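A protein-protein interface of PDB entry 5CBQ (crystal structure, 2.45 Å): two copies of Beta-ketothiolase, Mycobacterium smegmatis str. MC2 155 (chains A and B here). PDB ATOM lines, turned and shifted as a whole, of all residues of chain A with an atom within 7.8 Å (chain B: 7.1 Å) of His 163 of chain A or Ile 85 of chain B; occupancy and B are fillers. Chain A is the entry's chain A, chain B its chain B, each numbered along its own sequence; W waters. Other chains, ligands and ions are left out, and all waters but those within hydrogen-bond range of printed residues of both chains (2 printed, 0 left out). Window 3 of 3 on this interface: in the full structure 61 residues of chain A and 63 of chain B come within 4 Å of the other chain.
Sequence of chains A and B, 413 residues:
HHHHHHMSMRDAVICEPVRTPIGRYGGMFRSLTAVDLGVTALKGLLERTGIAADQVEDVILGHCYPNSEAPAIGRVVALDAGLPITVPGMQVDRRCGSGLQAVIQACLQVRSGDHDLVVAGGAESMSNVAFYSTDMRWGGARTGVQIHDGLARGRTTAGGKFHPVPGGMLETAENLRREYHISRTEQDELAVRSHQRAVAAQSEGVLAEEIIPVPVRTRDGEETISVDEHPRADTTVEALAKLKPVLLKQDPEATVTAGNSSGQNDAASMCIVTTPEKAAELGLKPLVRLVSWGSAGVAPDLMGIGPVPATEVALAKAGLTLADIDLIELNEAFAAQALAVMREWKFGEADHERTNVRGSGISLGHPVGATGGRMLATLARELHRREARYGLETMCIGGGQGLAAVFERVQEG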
ATOM      1  N   ARG A 155      20.743 -13.868  25.049  1.00  0.00           N
ATOM      2  CA  ARG A 155      20.714 -15.093  24.292  1.00  0.00           C
ATOM      3  C   ARG A 155      19.993 -16.241  24.954  1.00  0.00           C
ATOM      4  O   ARG A 155      19.662 -17.200  24.318  1.00  0.00           O
ATOM      5  CB  ARG A 155      22.104 -15.460  23.882  1.00  0.00           C
ATOM      6  CG  ARG A 155      22.770 -14.272  23.266  1.00  0.00           C
ATOM      7  CD  ARG A 155      24.062 -14.601  22.583  1.00  0.00           C
ATOM      8  NE  ARG A 155      25.024 -13.543  22.757  1.00  0.00           N
ATOM      9  CZ  ARG A 155      26.233 -13.748  23.222  1.00  0.00           C
ATOM     10  NH1 ARG A 155      26.590 -14.956  23.548  1.00  0.00           N
ATOM     11  NH2 ARG A 155      27.064 -12.754  23.371  1.00  0.00           N
ATOM     12  N   THR A 156      19.767 -16.130  26.241  1.00  0.00           N
ATOM     13  CA  THR A 156      19.096 -17.205  26.965  1.00  0.00           C
ATOM     14  C   THR A 156      17.657 -16.908  27.373  1.00  0.00           C
ATOM     15  O   THR A 156      16.816 -17.781  27.411  1.00  0.00           O
ATOM     16  CB  THR A 156      19.946 -17.693  28.151  1.00  0.00           C
ATOM     17  OG1 THR A 156      19.865 -16.778  29.215  1.00  0.00           O
ATOM     18  CG2 THR A 156      21.353 -17.743  27.762  1.00  0.00           C
ATOM     19  N   THR A 157      17.399 -15.646  27.663  1.00  0.00           N
ATOM     20  CA  THR A 157      16.098 -15.192  28.101  1.00  0.00           C
ATOM     21  C   THR A 157      14.961 -15.140  27.105  1.00  0.00           C
ATOM     22  O   THR A 157      13.835 -15.161  27.484  1.00  0.00           O
ATOM     23  CB  THR A 157      16.201 -13.945  28.963  1.00  0.00           C
ATOM     24  OG1 THR A 157      16.805 -12.880  28.239  1.00  0.00           O
ATOM     25  CG2 THR A 157      17.039 -14.250  30.105  1.00  0.00           C
ATOM     26  N   ALA A 158      15.257 -15.146  25.835  1.00  0.00           N
ATOM     27  CA  ALA A 158      14.243 -14.890  24.842  1.00  0.00           C
ATOM     28  C   ALA A 158      13.111 -15.865  24.796  1.00  0.00           C
ATOM     29  O   ALA A 158      12.047 -15.532  24.359  1.00  0.00           O
ATOM     30  CB  ALA A 158      14.841 -14.710  23.469  1.00  0.00           C
ATOM     31  N   GLY A 159      13.341 -17.080  25.223  1.00  0.00           N
ATOM     32  CA  GLY A 159      12.315 -18.078  25.149  1.00  0.00           C
ATOM     33  C   GLY A 159      11.460 -18.075  26.361  1.00  0.00           C
ATOM     34  O   GLY A 159      10.505 -18.760  26.404  1.00  0.00           O
ATOM     35  N   GLY A 160      11.836 -17.316  27.355  1.00  0.00           N
ATOM     36  CA  GLY A 160      11.157 -17.370  28.611  1.00  0.00           C
ATOM     37  C   GLY A 160      11.531 -18.570  29.463  1.00  0.00           C
ATOM     38  O   GLY A 160      12.359 -19.355  29.121  1.00  0.00           O
ATOM     39  N   LYS A 161      10.890 -18.717  30.595  1.00  0.00           N
ATOM     40  CA  LYS A 161      11.218 -19.778  31.509  1.00  0.00           C
ATOM     41  C   LYS A 161      10.985 -21.171  31.071  1.00  0.00           C
ATOM     42  O   LYS A 161      11.690 -22.026  31.479  1.00  0.00           O
ATOM     43  CB  LYS A 161      10.591 -19.561  32.860  1.00  0.00           C
ATOM     44  CG  LYS A 161       9.128 -19.299  32.884  1.00  0.00           C
ATOM     45  CD  LYS A 161       8.846 -18.633  34.196  1.00  0.00           C
ATOM     46  CE  LYS A 161       7.448 -18.941  34.645  1.00  0.00           C
ATOM     47  NZ  LYS A 161       7.241 -18.525  36.047  1.00  0.00           N
ATOM     48  N   PHE A 162       9.943 -21.415  30.325  1.00  0.00           N
ATOM     49  CA  PHE A 162       9.644 -22.748  29.863  1.00  0.00           C
ATOM     50  C   PHE A 162      10.525 -23.256  28.792  1.00  0.00           C
ATOM     51  O   PHE A 162      10.638 -24.432  28.624  1.00  0.00           O
ATOM     52  CB  PHE A 162       8.190 -22.926  29.524  1.00  0.00           C
ATOM     53  CG  PHE A 162       7.318 -22.631  30.656  1.00  0.00           C
ATOM     54  CD1 PHE A 162       7.529 -23.251  31.835  1.00  0.00           C
ATOM     55  CD2 PHE A 162       6.342 -21.677  30.567  1.00  0.00           C
ATOM     56  CE1 PHE A 162       6.765 -22.957  32.926  1.00  0.00           C
ATOM     57  CE2 PHE A 162       5.566 -21.374  31.649  1.00  0.00           C
ATOM     58  CZ  PHE A 162       5.779 -22.017  32.838  1.00  0.00           C
ATOM     59  N   HIS A 163      11.115 -22.365  28.041  1.00  0.00           N
ATOM     60  CA  HIS A 163      12.017 -22.787  27.019  1.00  0.00           C
ATOM     61  C   HIS A 163      13.289 -21.991  27.108  1.00  0.00           C
ATOM     62  O   HIS A 163      13.564 -21.172  26.260  1.00  0.00           O
ATOM     63  CB  HIS A 163      11.389 -22.653  25.652  1.00  0.00           C
ATOM     64  CG  HIS A 163       9.922 -22.902  25.628  1.00  0.00           C
ATOM     65  ND1 HIS A 163       9.352 -23.893  24.881  1.00  0.00           N
ATOM     66  CD2 HIS A 163       8.906 -22.268  26.237  1.00  0.00           C
ATOM     67  CE1 HIS A 163       8.046 -23.864  25.036  1.00  0.00           C
ATOM     68  NE2 HIS A 163       7.752 -22.892  25.862  1.00  0.00           N
ATOM     69  N   PRO A 164      14.072 -22.198  28.147  1.00  0.00           N
ATOM     70  CA  PRO A 164      15.390 -21.603  28.192  1.00  0.00           C
ATOM     71  C   PRO A 164      16.292 -22.302  27.205  1.00  0.00           C
ATOM     72  O   PRO A 164      16.127 -23.475  26.965  1.00  0.00           O
ATOM     73  CB  PRO A 164      15.827 -21.886  29.609  1.00  0.00           C
ATOM     74  CG  PRO A 164      15.137 -23.141  29.971  1.00  0.00           C
ATOM     75  CD  PRO A 164      13.958 -23.315  29.084  1.00  0.00           C
ATOM     76  N   VAL A 165      17.199 -21.576  26.586  1.00  0.00           N
ATOM     77  CA  VAL A 165      18.174 -22.196  25.728  1.00  0.00           C
ATOM     78  C   VAL A 165      19.485 -21.678  26.202  1.00  0.00           C
ATOM     79  O   VAL A 165      19.850 -20.610  25.848  1.00  0.00           O
ATOM     80  CB  VAL A 165      17.943 -21.848  24.264  1.00  0.00           C
ATOM     81  CG1 VAL A 165      19.119 -22.266  23.432  1.00  0.00           C
ATOM     82  CG2 VAL A 165      16.714 -22.556  23.737  1.00  0.00           C
ATOM     83  N   PRO A 166      20.183 -22.403  27.064  1.00  0.00           N
ATOM     84  CA  PRO A 166      21.399 -21.902  27.714  1.00  0.00           C
ATOM     85  C   PRO A 166      22.531 -21.675  26.758  1.00  0.00           C
ATOM     86  O   PRO A 166      23.413 -20.880  26.990  1.00  0.00           O
ATOM     87  CB  PRO A 166      21.755 -22.999  28.679  1.00  0.00           C
ATOM     88  CG  PRO A 166      20.579 -23.890  28.714  1.00  0.00           C
ATOM     89  CD  PRO A 166      19.984 -23.817  27.368  1.00  0.00           C
ATOM     90  N   ALA A 296       5.148 -15.518  12.265  1.00  0.00           N
ATOM     91  CA  ALA A 296       4.924 -16.852  12.763  1.00  0.00           C
ATOM     92  C   ALA A 296       5.613 -17.073  14.054  1.00  0.00           C
ATOM     93  O   ALA A 296       6.537 -16.405  14.362  1.00  0.00           O
ATOM     94  CB  ALA A 296       5.438 -17.852  11.770  1.00  0.00           C
ATOM     95  N   GLY A 297       5.180 -18.069  14.783  1.00  0.00           N
ATOM     96  CA  GLY A 297       5.926 -18.551  15.913  1.00  0.00           C
ATOM     97  C   GLY A 297       6.392 -19.989  15.813  1.00  0.00           C
ATOM     98  O   GLY A 297       5.732 -20.818  15.301  1.00  0.00           O
ATOM     99  N   VAL A 298       7.561 -20.268  16.334  1.00  0.00           N
ATOM    100  CA  VAL A 298       8.135 -21.585  16.270  1.00  0.00           C
ATOM    101  C   VAL A 298       8.779 -21.805  17.590  1.00  0.00           C
ATOM    102  O   VAL A 298       8.927 -20.895  18.327  1.00  0.00           O
ATOM    103  CB  VAL A 298       9.214 -21.728  15.206  1.00  0.00           C
ATOM    104  CG1 VAL A 298       8.647 -21.712  13.818  1.00  0.00           C
ATOM    105  CG2 VAL A 298      10.305 -20.726  15.389  1.00  0.00           C
ATOM    106  N   ALA A 299       9.197 -23.015  17.866  1.00  0.00           N
ATOM    107  CA  ALA A 299       9.875 -23.306  19.090  1.00  0.00           C
ATOM    108  C   ALA A 299      11.137 -22.541  19.214  1.00  0.00           C
ATOM    109  O   ALA A 299      11.885 -22.447  18.300  1.00  0.00           O
ATOM    110  CB  ALA A 299      10.205 -24.765  19.128  1.00  0.00           C
ATOM    111  N   PRO A 300      11.432 -22.072  20.400  1.00  0.00           N
ATOM    112  CA  PRO A 300      12.646 -21.321  20.615  1.00  0.00           C
ATOM    113  C   PRO A 300      13.880 -22.115  20.337  1.00  0.00           C
ATOM    114  O   PRO A 300      14.779 -21.554  19.788  1.00  0.00           O
ATOM    115  CB  PRO A 300      12.579 -21.000  22.080  1.00  0.00           C
ATOM    116  CG  PRO A 300      11.158 -20.863  22.329  1.00  0.00           C
ATOM    117  CD  PRO A 300      10.470 -21.856  21.474  1.00  0.00           C
ATOM    118  N   ASP A 301      13.947 -23.386  20.704  1.00  0.00           N
ATOM    119  CA  ASP A 301      15.153 -24.166  20.490  1.00  0.00           C
ATOM    120  C   ASP A 301      15.321 -24.472  19.019  1.00  0.00           C
ATOM    121  O   ASP A 301      16.340 -24.923  18.592  1.00  0.00           O
ATOM    122  CB  ASP A 301      15.233 -25.380  21.402  1.00  0.00           C
ATOM    123  CG  ASP A 301      14.182 -26.386  21.130  1.00  0.00           C
ATOM    124  OD1 ASP A 301      13.513 -26.283  20.128  1.00  0.00           O
ATOM    125  OD2 ASP A 301      14.020 -27.302  21.926  1.00  0.00           O
ATOM    126  N   GLY A 399      14.067 -16.290  20.065  1.00  0.00           N
ATOM    127  CA  GLY A 399      12.912 -16.553  20.869  1.00  0.00           C
ATOM    128  C   GLY A 399      11.866 -17.323  20.151  1.00  0.00           C
ATOM    129  O   GLY A 399      10.867 -17.652  20.711  1.00  0.00           O
ATOM    130  N   GLY A 400      12.122 -17.652  18.911  1.00  0.00           N
ATOM    131  CA  GLY A 400      11.197 -18.424  18.133  1.00  0.00           C
ATOM    132  C   GLY A 400      10.176 -17.692  17.330  1.00  0.00           C
ATOM    133  O   GLY A 400       9.019 -17.909  17.448  1.00  0.00           O
ATOM    134  N   GLN A 401      10.636 -16.832  16.458  1.00  0.00           N
ATOM    135  CA  GLN A 401       9.764 -16.065  15.609  1.00  0.00           C
ATOM    136  C   GLN A 401      10.270 -15.996  14.197  1.00  0.00           C
ATOM    137  O   GLN A 401      11.380 -16.271  13.936  1.00  0.00           O
ATOM    138  CB  GLN A 401       9.567 -14.674  16.172  1.00  0.00           C
ATOM    139  CG  GLN A 401       8.619 -14.616  17.337  1.00  0.00           C
ATOM    140  CD  GLN A 401       8.216 -13.237  17.722  1.00  0.00           C
ATOM    141  OE1 GLN A 401       7.257 -12.747  17.252  1.00  0.00           O
ATOM    142  NE2 GLN A 401       8.931 -12.639  18.596  1.00  0.00           N
ATOM    143  N   ARG B  75       6.379 -11.581  23.241  1.00  0.00           N
ATOM    144  CA  ARG B  75       6.638 -12.980  23.035  1.00  0.00           C
ATOM    145  C   ARG B  75       6.938 -13.753  24.313  1.00  0.00           C
ATOM    146  O   ARG B  75       6.437 -14.802  24.477  1.00  0.00           O
ATOM    147  CB  ARG B  75       7.708 -13.157  21.964  1.00  0.00           C
ATOM    148  CG  ARG B  75       8.407 -14.484  21.913  1.00  0.00           C
ATOM    149  CD  ARG B  75       7.508 -15.494  21.301  1.00  0.00           C
ATOM    150  NE  ARG B  75       8.244 -16.615  20.812  1.00  0.00           N
ATOM    151  CZ  ARG B  75       7.734 -17.661  20.216  1.00  0.00           C
ATOM    152  NH1 ARG B  75       6.473 -17.776  19.978  1.00  0.00           N
ATOM    153  NH2 ARG B  75       8.527 -18.599  19.853  1.00  0.00           N
ATOM    154  N   LEU B  79       4.544 -16.850  26.059  1.00  0.00           N
ATOM    155  CA  LEU B  79       5.133 -18.094  26.385  1.00  0.00           C
ATOM    156  C   LEU B  79       5.011 -18.444  27.825  1.00  0.00           C
ATOM    157  O   LEU B  79       4.670 -19.540  28.126  1.00  0.00           O
ATOM    158  CB  LEU B  79       6.581 -18.123  25.928  1.00  0.00           C
ATOM    159  CG  LEU B  79       6.702 -18.262  24.424  1.00  0.00           C
ATOM    160  CD1 LEU B  79       8.075 -18.015  23.876  1.00  0.00           C
ATOM    161  CD2 LEU B  79       6.083 -19.519  23.899  1.00  0.00           C
ATOM    162  N   ASP B  80       5.303 -17.495  28.692  1.00  0.00           N
ATOM    163  CA  ASP B  80       5.252 -17.670  30.118  1.00  0.00           C
ATOM    164  C   ASP B  80       3.870 -17.851  30.629  1.00  0.00           C
ATOM    165  O   ASP B  80       3.666 -18.413  31.660  1.00  0.00           O
ATOM    166  CB  ASP B  80       5.989 -16.552  30.833  1.00  0.00           C
ATOM    167  CG  ASP B  80       7.477 -16.676  30.722  1.00  0.00           C
ATOM    168  OD1 ASP B  80       7.928 -17.443  29.880  1.00  0.00           O
ATOM    169  OD2 ASP B  80       8.202 -15.992  31.433  1.00  0.00           O
ATOM    170  N   GLY B  82       1.801 -19.606  28.960  1.00  0.00           N
ATOM    171  CA  GLY B  82       1.406 -20.876  28.444  1.00  0.00           C
ATOM    172  C   GLY B  82       0.734 -20.898  27.123  1.00  0.00           C
ATOM    173  O   GLY B  82       0.056 -21.834  26.807  1.00  0.00           O
ATOM    174  N   LEU B  83       0.911 -19.847  26.362  1.00  0.00           N
ATOM    175  CA  LEU B  83       0.456 -19.855  25.000  1.00  0.00           C
ATOM    176  C   LEU B  83       1.369 -20.711  24.161  1.00  0.00           C
ATOM    177  O   LEU B  83       2.518 -20.914  24.475  1.00  0.00           O
ATOM    178  CB  LEU B  83       0.324 -18.452  24.407  1.00  0.00           C
ATOM    179  CG  LEU B  83      -0.937 -17.691  24.737  1.00  0.00           C
ATOM    180  CD1 LEU B  83      -1.139 -17.775  26.222  1.00  0.00           C
ATOM    181  CD2 LEU B  83      -0.849 -16.240  24.338  1.00  0.00           C
ATOM    182  N   PRO B  84       0.863 -21.185  23.060  1.00  0.00           N
ATOM    183  CA  PRO B  84       1.615 -22.043  22.168  1.00  0.00           C
ATOM    184  C   PRO B  84       2.713 -21.292  21.435  1.00  0.00           C
ATOM    185  O   PRO B  84       2.625 -20.110  21.272  1.00  0.00           O
ATOM    186  CB  PRO B  84       0.555 -22.532  21.198  1.00  0.00           C
ATOM    187  CG  PRO B  84      -0.582 -21.601  21.343  1.00  0.00           C
ATOM    188  CD  PRO B  84      -0.561 -21.171  22.746  1.00  0.00           C
ATOM    189  N   ILE B  85       3.713 -21.997  20.965  1.00  0.00           N
ATOM    190  CA  ILE B  85       4.900 -21.417  20.408  1.00  0.00           C
ATOM    191  C   ILE B  85       4.598 -20.784  19.065  1.00  0.00           C
ATOM    192  O   ILE B  85       5.432 -20.158  18.483  1.00  0.00           O
ATOM    193  CB  ILE B  85       6.062 -22.428  20.331  1.00  0.00           C
ATOM    194  CG1 ILE B  85       5.573 -23.843  20.057  1.00  0.00           C
ATOM    195  CG2 ILE B  85       6.838 -22.434  21.619  1.00  0.00           C
ATOM    196  CD1 ILE B  85       5.356 -24.189  18.613  1.00  0.00           C
ATOM    197  N   THR B  86       3.373 -20.950  18.607  1.00  0.00           N
ATOM    198  CA  THR B  86       2.933 -20.441  17.330  1.00  0.00           C
ATOM    199  C   THR B  86       2.562 -18.981  17.363  1.00  0.00           C
ATOM    200  O   THR B  86       2.284 -18.407  16.343  1.00  0.00           O
ATOM    201  CB  THR B  86       1.720 -21.186  16.814  1.00  0.00           C
ATOM    202  OG1 THR B  86       0.875 -21.478  17.892  1.00  0.00           O
ATOM    203  CG2 THR B  86       2.113 -22.432  16.189  1.00  0.00           C
ATOM    204  N   VAL B  87       2.518 -18.431  18.560  1.00  0.00           N
ATOM    205  CA  VAL B  87       2.014 -17.112  18.793  1.00  0.00           C
ATOM    206  C   VAL B  87       3.151 -16.120  18.936  1.00  0.00           C
ATOM    207  O   VAL B  87       3.905 -16.183  19.856  1.00  0.00           O
ATOM    208  CB  VAL B  87       1.143 -17.078  20.051  1.00  0.00           C
ATOM    209  CG1 VAL B  87       0.728 -15.674  20.376  1.00  0.00           C
ATOM    210  CG2 VAL B  87      -0.068 -17.946  19.893  1.00  0.00           C
ATOM    211  N   PRO B  88       3.275 -15.198  18.007  1.00  0.00           N
ATOM    212  CA  PRO B  88       4.313 -14.178  18.045  1.00  0.00           C
ATOM    213  C   PRO B  88       3.995 -13.001  18.942  1.00  0.00           C
ATOM    214  O   PRO B  88       2.884 -12.838  19.293  1.00  0.00           O
ATOM    215  CB  PRO B  88       4.439 -13.752  16.594  1.00  0.00           C
ATOM    216  CG  PRO B  88       3.463 -14.539  15.846  1.00  0.00           C
ATOM    217  CD  PRO B  88       2.473 -15.058  16.813  1.00  0.00           C
HETATM  218  O   HOH W   1       4.865 -16.888  34.403  1.00  0.00           O
HETATM  219  O   HOH W   2       8.334 -19.525  28.502  1.00  0.00           O
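Of the 21 printed residues of chain A, 12 touch a printed residue of chain B.
Hydrophobic or aromatic side chains of chain A within 4 Å of the printed part of chain B: Phe 162, His 163 and Pro 300.
Along chain A the printed residues that touch a printed residue of chain B span positions 159 to 401.
Of the 10 printed residues of chain B, 6 touch a printed residue of chain A.
Hydrophobic or aromatic side chains of chain B that line the printed part of chain A: Leu 79, Ile 85 and Pro 88.
The backbone carbonyl oxygen (O) of Ile 85 of chain B is in hydrogen-bond range of the guanidinium group (NH1) of Arg 75 of chain B (3.0 Å).
The guanidinium group (NH1) of Arg 75 of chain B lies within hydrogen-bond range of the backbone carbonyl oxygen (O) of Val 87 of chain B, 3.0 Å away.
The backbone carbonyl oxygen of Gly 400 of chain A sits at hydrogen-bond distance from the backbone NH of Val 298 of chain A (3.0 Å).
No position is printed for both chains.
Of the 16 pairs that touch across the chains among the printed residues, none has its exchanged pair printed and touching as well.
Gly 159 of chain A touches Leu 79 of chain B (O to CD1, 3.6 Å).
CA of Gly 160 of chain A touches OD1 of Asp 80 of chain B, 3.5 Å away.
CD2 of Phe 162 of chain A touches O of Leu 79 of chain B, at 3.6 Å.
CE2 of Phe 162 of chain A touches O of Asp 80 of chain B, 3.5 Å away.
Ile 85 of chain B touches His 163 of chain A (CG2 to CE1, 3.9 Å).
Ala 296 of chain A touches Pro 88 of chain B.
Ile 85 of chain B touches Pro 300 of chain A (CG2 to CD, 3.7 Å).
CB of Arg 75 of chain B touches NE2 of Gln 401 of chain A, 3.6 Å away.
OE1 of Gln 401 of chain A touches CB of Pro 88 of chain B, at 3.1 Å.
Water W2 lies within hydrogen-bond range of the side-chain carboxylate (OD1) of Asp 80 of chain B, the backbone NH (N) of Phe 162 of chain A, the backbone carbonyl oxygen (O) of Gly 159 of chain A and the backbone NH (N) of Lys 161 of chain A.
Water W1 bridges the side-chain amino group of Lys 161 of chain A (3.3 Å) and the backbone carbonyl oxygen of Asp 80 of chain B (3.4 Å).
Of chain B, only Ile 85 (3.9 Å) comes within 4 Å of His 163 of chain A.
Ile 85 of chain B touches just these residues of chain A: His 163 (3.9 Å), Gly 297 (2.8 Å), Val 298 (3.0 Å) and Pro 300 (3.7 Å).
Printed residues of chain B within 4 Å of Gly 399 of chain A: Arg 75 (2.7 Å).
Printed residues of chain A within 4 Å of Arg 75 of chain B: Val 298 (2.8 Å), Gly 399 (2.7 Å), Gly 400 (2.5 Å) and Gln 401 (3.6 Å).
Of the printed residues of chain A, Pro 88 of chain B touches Ala 296 and Gln 401.
The nearest residue of chain B that does not touch His 163 of chain A is Leu 79 of chain B (4.2 Å).
N of Gly 297 of chain A sits at hydrogen-bond distance from O of Thr 86 of chain B, 3.3 Å away.
The backbone carbonyl oxygen (O) of Gly 399 of chain A is in hydrogen-bond range of the guanidinium group (NH2) of Arg 75 of chain B.
O of Ile 85 of chain B lies within hydrogen-bond range of N of Val 298 of chain A.
The backbone carbonyl oxygen (O) of Ile 85 of chain B sits close to the backbone carbonyl oxygen (O) of Gly 297 of chain A (3.3 Å).
The side-chain carboxylate (OD1) of Asp 80 of chain B lies within hydrogen-bond range of the backbone NH (N) of Lys 161 of chain A.
The backbone carbonyl oxygen (O) of Gly 400 of chain A is in hydrogen-bond range of the guanidinium group (NH2) of Arg 75 of chain B (2.5 Å).
O of Val 298 of chain A is in hydrogen-bond range of NH2 of Arg 75 of chain B (2.8 Å).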
